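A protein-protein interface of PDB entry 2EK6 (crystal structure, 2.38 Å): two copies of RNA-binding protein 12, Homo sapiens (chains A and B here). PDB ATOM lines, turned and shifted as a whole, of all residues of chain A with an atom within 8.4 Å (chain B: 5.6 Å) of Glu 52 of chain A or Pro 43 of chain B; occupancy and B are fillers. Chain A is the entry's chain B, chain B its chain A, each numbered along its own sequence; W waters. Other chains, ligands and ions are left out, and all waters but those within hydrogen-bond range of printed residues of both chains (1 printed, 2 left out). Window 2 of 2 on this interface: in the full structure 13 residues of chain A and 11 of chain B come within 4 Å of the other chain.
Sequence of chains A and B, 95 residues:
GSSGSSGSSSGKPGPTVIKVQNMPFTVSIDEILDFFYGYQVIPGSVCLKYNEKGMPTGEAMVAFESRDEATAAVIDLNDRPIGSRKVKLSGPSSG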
ATOM      1  N   LYS A  49     -30.522  20.715  15.759  1.00  0.00           N
ATOM      2  CA  LYS A  49     -29.867  20.734  17.068  1.00  0.00           C
ATOM      3  C   LYS A  49     -30.797  20.658  18.270  1.00  0.00           C
ATOM      4  O   LYS A  49     -31.925  21.130  18.220  1.00  0.00           O
ATOM      5  CB  LYS A  49     -28.981  21.977  17.174  1.00  0.00           C
ATOM      6  CG  LYS A  49     -27.995  22.100  16.014  1.00  0.00           C
ATOM      7  CD  LYS A  49     -26.921  23.135  16.300  1.00  0.00           C
ATOM      8  CE  LYS A  49     -26.169  22.777  17.569  1.00  0.00           C
ATOM      9  NZ  LYS A  49     -24.950  23.592  17.796  1.00  0.00           N
ATOM     10  N   TYR A  50     -30.298  20.065  19.353  1.00  0.00           N
ATOM     11  CA  TYR A  50     -31.057  19.902  20.594  1.00  0.00           C
ATOM     12  C   TYR A  50     -30.187  20.316  21.766  1.00  0.00           C
ATOM     13  O   TYR A  50     -28.965  20.188  21.700  1.00  0.00           O
ATOM     14  CB  TYR A  50     -31.453  18.426  20.796  1.00  0.00           C
ATOM     15  CG  TYR A  50     -32.258  17.847  19.663  1.00  0.00           C
ATOM     16  CD1 TYR A  50     -31.663  17.558  18.431  1.00  0.00           C
ATOM     17  CD2 TYR A  50     -33.639  17.691  19.785  1.00  0.00           C
ATOM     18  CE1 TYR A  50     -32.425  17.142  17.350  1.00  0.00           C
ATOM     19  CE2 TYR A  50     -34.414  17.280  18.709  1.00  0.00           C
ATOM     20  CZ  TYR A  50     -33.800  17.005  17.495  1.00  0.00           C
ATOM     21  OH  TYR A  50     -34.551  16.571  16.430  1.00  0.00           O
ATOM     22  N   ASN A  51     -30.815  20.783  22.845  1.00  0.00           N
ATOM     23  CA  ASN A  51     -30.073  21.165  24.041  1.00  0.00           C
ATOM     24  C   ASN A  51     -29.925  19.929  24.929  1.00  0.00           C
ATOM     25  O   ASN A  51     -30.345  18.839  24.545  1.00  0.00           O
ATOM     26  CB  ASN A  51     -30.787  22.297  24.797  1.00  0.00           C
ATOM     27  CG  ASN A  51     -32.277  22.070  24.935  1.00  0.00           C
ATOM     28  OD1 ASN A  51     -32.727  20.941  25.123  1.00  0.00           O
ATOM     29  ND2 ASN A  51     -33.053  23.152  24.861  1.00  0.00           N
ATOM     30  N   GLU A  52     -29.328  20.087  26.107  1.00  0.00           N
ATOM     31  CA  GLU A  52     -29.140  18.950  26.999  1.00  0.00           C
ATOM     32  C   GLU A  52     -30.442  18.435  27.581  1.00  0.00           C
ATOM     33  O   GLU A  52     -30.452  17.429  28.294  1.00  0.00           O
ATOM     34  CB  GLU A  52     -28.173  19.281  28.143  1.00  0.00           C
ATOM     35  CG  GLU A  52     -28.502  20.518  28.950  1.00  0.00           C
ATOM     36  CD  GLU A  52     -28.002  21.780  28.284  1.00  0.00           C
ATOM     37  OE1 GLU A  52     -28.683  22.275  27.351  1.00  0.00           O
ATOM     38  OE2 GLU A  52     -26.916  22.264  28.694  1.00  0.00           O
ATOM     39  N   LYS A  53     -31.536  19.129  27.291  1.00  0.00           N
ATOM     40  CA  LYS A  53     -32.835  18.697  27.776  1.00  0.00           C
ATOM     41  C   LYS A  53     -33.499  17.856  26.696  1.00  0.00           C
ATOM     42  O   LYS A  53     -34.511  17.195  26.943  1.00  0.00           O
ATOM     43  CB  LYS A  53     -33.706  19.901  28.167  1.00  0.00           C
ATOM     44  CG  LYS A  53     -33.275  20.506  29.494  1.00  0.00           C
ATOM     45  CD  LYS A  53     -34.286  21.486  30.070  1.00  0.00           C
ATOM     46  CE  LYS A  53     -34.210  22.851  29.406  1.00  0.00           C
ATOM     47  NZ  LYS A  53     -35.112  23.848  30.078  1.00  0.00           N
ATOM     48  N   GLY A  54     -32.900  17.871  25.506  1.00  0.00           N
ATOM     49  CA  GLY A  54     -33.413  17.095  24.392  1.00  0.00           C
ATOM     50  C   GLY A  54     -34.508  17.797  23.614  1.00  0.00           C
ATOM     51  O   GLY A  54     -35.236  17.170  22.835  1.00  0.00           O
ATOM     52  N   MET A  55     -34.616  19.108  23.814  1.00  0.00           N
ATOM     53  CA  MET A  55     -35.645  19.888  23.144  1.00  0.00           C
ATOM     54  C   MET A  55     -35.164  20.676  21.932  1.00  0.00           C
ATOM     55  O   MET A  55     -33.999  21.034  21.840  1.00  0.00           O
ATOM     56  CB  MET A  55     -36.323  20.807  24.159  1.00  0.00           C
ATOM     57  CG  MET A  55     -37.056  20.041  25.248  1.00  0.00           C
ATOM     58  SD  MET A  55     -38.292  18.846  24.623  1.00  0.00           S
ATOM     59  CE  MET A  55     -39.594  20.007  24.133  1.00  0.00           C
ATOM     60  N   THR A  57     -34.077  23.437  19.446  1.00  0.00           N
ATOM     61  CA  THR A  57     -33.457  24.761  19.655  1.00  0.00           C
ATOM     62  C   THR A  57     -33.770  25.835  18.596  1.00  0.00           C
ATOM     63  O   THR A  57     -33.558  27.027  18.829  1.00  0.00           O
ATOM     64  CB  THR A  57     -31.899  24.660  19.732  1.00  0.00           C
ATOM     65  OG1 THR A  57     -31.506  23.933  20.905  1.00  0.00           O
ATOM     66  CG2 THR A  57     -31.278  26.044  19.764  1.00  0.00           C
ATOM     67  N   ILE B  29     -32.474  11.730  22.626  1.00  0.00           N
ATOM     68  CA  ILE B  29     -31.299  12.478  22.921  1.00  0.00           C
ATOM     69  C   ILE B  29     -30.644  11.871  24.186  1.00  0.00           C
ATOM     70  O   ILE B  29     -29.413  11.699  24.254  1.00  0.00           O
ATOM     71  CB  ILE B  29     -31.694  13.987  23.022  1.00  0.00           C
ATOM     72  CG1 ILE B  29     -31.981  14.521  21.598  1.00  0.00           C
ATOM     73  CG2 ILE B  29     -30.609  14.808  23.749  1.00  0.00           C
ATOM     74  CD1 ILE B  29     -30.793  14.480  20.635  1.00  0.00           C
ATOM     75  N   ASP B  30     -31.462  11.508  25.169  1.00  0.00           N
ATOM     76  CA  ASP B  30     -30.951  10.888  26.379  1.00  0.00           C
ATOM     77  C   ASP B  30     -30.121   9.640  26.023  1.00  0.00           C
ATOM     78  O   ASP B  30     -29.020   9.451  26.544  1.00  0.00           O
ATOM     79  CB  ASP B  30     -32.118  10.492  27.303  1.00  0.00           C
ATOM     80  CG  ASP B  30     -32.777  11.700  27.982  1.00  0.00           C
ATOM     81  OD1 ASP B  30     -32.045  12.626  28.393  1.00  0.00           O
ATOM     82  OD2 ASP B  30     -34.025  11.711  28.133  1.00  0.00           O
ATOM     83  N   LEU B  33     -26.584  10.412  24.566  1.00  0.00           N
ATOM     84  CA  LEU B  33     -25.711  10.923  25.614  1.00  0.00           C
ATOM     85  C   LEU B  33     -25.296   9.782  26.537  1.00  0.00           C
ATOM     86  O   LEU B  33     -24.131   9.677  26.925  1.00  0.00           O
ATOM     87  CB  LEU B  33     -26.434  12.019  26.409  1.00  0.00           C
ATOM     88  CG  LEU B  33     -26.750  13.300  25.629  1.00  0.00           C
ATOM     89  CD1 LEU B  33     -27.574  14.256  26.485  1.00  0.00           C
ATOM     90  CD2 LEU B  33     -25.459  13.958  25.207  1.00  0.00           C
ATOM     91  N   VAL B  41     -18.508  14.343  26.981  1.00  0.00           N
ATOM     92  CA  VAL B  41     -19.349  14.840  25.909  1.00  0.00           C
ATOM     93  C   VAL B  41     -20.124  16.069  26.347  1.00  0.00           C
ATOM     94  O   VAL B  41     -20.470  16.223  27.521  1.00  0.00           O
ATOM     95  CB  VAL B  41     -20.341  13.750  25.415  1.00  0.00           C
ATOM     96  CG1 VAL B  41     -21.175  13.224  26.567  1.00  0.00           C
ATOM     97  CG2 VAL B  41     -21.246  14.320  24.326  1.00  0.00           C
ATOM     98  N   ILE B  42     -20.374  16.943  25.377  1.00  0.00           N
ATOM     99  CA  ILE B  42     -21.105  18.186  25.573  1.00  0.00           C
ATOM    100  C   ILE B  42     -22.597  17.895  25.370  1.00  0.00           C
ATOM    101  O   ILE B  42     -23.043  17.624  24.253  1.00  0.00           O
ATOM    102  CB  ILE B  42     -20.600  19.241  24.564  1.00  0.00           C
ATOM    103  CG1 ILE B  42     -19.122  19.539  24.839  1.00  0.00           C
ATOM    104  CG2 ILE B  42     -21.430  20.505  24.660  1.00  0.00           C
ATOM    105  CD1 ILE B  42     -18.455  20.417  23.803  1.00  0.00           C
ATOM    106  N   PRO B  43     -23.387  17.957  26.462  1.00  0.00           N
ATOM    107  CA  PRO B  43     -24.838  17.706  26.529  1.00  0.00           C
ATOM    108  C   PRO B  43     -25.755  18.387  25.515  1.00  0.00           C
ATOM    109  O   PRO B  43     -26.764  17.812  25.113  1.00  0.00           O
ATOM    110  CB  PRO B  43     -25.196  18.114  27.955  1.00  0.00           C
ATOM    111  CG  PRO B  43     -23.951  17.903  28.697  1.00  0.00           C
ATOM    112  CD  PRO B  43     -22.910  18.456  27.763  1.00  0.00           C
ATOM    113  N   GLY B  44     -25.427  19.616  25.128  1.00  0.00           N
ATOM    114  CA  GLY B  44     -26.249  20.330  24.170  1.00  0.00           C
ATOM    115  C   GLY B  44     -25.539  20.544  22.849  1.00  0.00           C
ATOM    116  O   GLY B  44     -25.665  21.604  22.236  1.00  0.00           O
ATOM    117  N   SER B  45     -24.794  19.528  22.417  1.00  0.00           N
ATOM    118  CA  SER B  45     -24.039  19.576  21.169  1.00  0.00           C
ATOM    119  C   SER B  45     -24.584  18.634  20.093  1.00  0.00           C
ATOM    120  O   SER B  45     -24.112  18.661  18.949  1.00  0.00           O
ATOM    121  CB  SER B  45     -22.572  19.218  21.436  1.00  0.00           C
ATOM    122  OG  SER B  45     -22.451  17.867  21.845  1.00  0.00           O
ATOM    123  N   VAL B  46     -25.568  17.810  20.461  1.00  0.00           N
ATOM    124  CA  VAL B  46     -26.158  16.839  19.542  1.00  0.00           C
ATOM    125  C   VAL B  46     -27.126  17.429  18.555  1.00  0.00           C
ATOM    126  O   VAL B  46     -28.073  18.146  18.892  1.00  0.00           O
ATOM    127  CB  VAL B  46     -26.863  15.700  20.278  1.00  0.00           C
ATOM    128  CG1 VAL B  46     -27.506  14.751  19.270  1.00  0.00           C
ATOM    129  CG2 VAL B  46     -25.852  14.964  21.135  1.00  0.00           C
ATOM    130  N   GLU B  65     -15.519  17.878  25.025  1.00  0.00           N
ATOM    131  CA  GLU B  65     -14.775  18.981  25.640  1.00  0.00           C
ATOM    132  C   GLU B  65     -13.359  19.142  25.081  1.00  0.00           C
ATOM    133  O   GLU B  65     -12.771  20.224  25.156  1.00  0.00           O
ATOM    134  CB  GLU B  65     -14.698  18.800  27.163  1.00  0.00           C
ATOM    135  CG  GLU B  65     -16.040  18.600  27.857  1.00  0.00           C
ATOM    136  CD  GLU B  65     -16.815  19.875  28.045  1.00  0.00           C
ATOM    137  OE1 GLU B  65     -16.362  20.921  27.530  1.00  0.00           O
ATOM    138  OE2 GLU B  65     -17.880  19.827  28.704  1.00  0.00           O
HETATM  139  O   HOH W   1     -24.630  21.379  27.201  1.00  0.00           O
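No position is printed for both chains. Of the 9 pairs that touch across the chains among the printed residues, none has its exchanged pair printed and touching as well.
Water W1 bridges the backbone NH of Gly 44 of chain B (2.8 Å) and the side-chain carboxylate of Glu 52 of chain A (2.9 Å).
O of Lys 49 of chain A is in hydrogen-bond range of N of Thr 57 of chain A (3.4 Å). The side-chain amide oxygen (OD1) of Asn 51 of chain A sits close to the backbone NH (N) of Lys 53 of chain A (3.1 Å). OD1 of Asn 51 of chain A lies within hydrogen-bond range of N of Gly 54 of chain A. The side-chain amide oxygen (OD1) of Asn 51 of chain A lies within hydrogen-bond range of the backbone NH (N) of Met 55 of chain A (2.9 Å).
N of Tyr 50 of chain A is in hydrogen-bond range of O of Val 46 of chain B (3.0 Å).
Lys 49 of chain A touches Val 46 of chain B (CA to O, 3.6 Å). Ile 29 of chain B touches Tyr 50 of chain A. O of Tyr 50 of chain A touches O of Gly 44 of chain B (3.6 Å). O of Asn 51 of chain A touches O of Pro 43 of chain B (3.8 Å). C of Asn 51 of chain A touches CA of Gly 44 of chain B (3.8 Å). CB of Pro 43 of chain B touches CB of Glu 52 of chain A, 3.2 Å away. Glu 52 of chain A touches Gly 44 of chain B. CA of Gly 54 of chain A touches CG2 of Ile 29 of chain B, 3.7 Å away.
Of the printed residues of chain B, Tyr 50 of chain A touches Ile 29, Gly 44 and Val 46. Glu 52 of chain A touches two residues of chain B. Of the printed residues of chain B, Gly 54 of chain A touches Ile 29. Of the printed residues of chain A, Ile 29 of chain B touches Tyr 50 (3.8 Å) and Gly 54 (3.7 Å). Asp 30 of chain B touches none of the printed residues of chain A. Of the printed residues of chain A, Pro 43 of chain B touches Asn 51 and Glu 52. Printed residues of chain A within 4 Å of Val 46 of chain B: Lys 49 and Tyr 50. The nearest residue of chain A that does not touch Pro 43 of chain B is Tyr 50 of chain A (4.7 Å).
Hydrophobic or aromatic side chains of chain B within 4 Å of the printed part of chain A: Ile 29 and Pro 43. Printed residues of chain A that touch a printed residue of chain B: Lys 49, Tyr 50, Asn 51, Glu 52 and Gly 54. Hydrophobic or aromatic side chains of chain A within 4 Å of the printed part of chain B: Tyr 50. Among the printed residues, no Asp or Glu carboxylate lies within 4 Å of a Lys or Arg side-chain nitrogen of the other chain.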
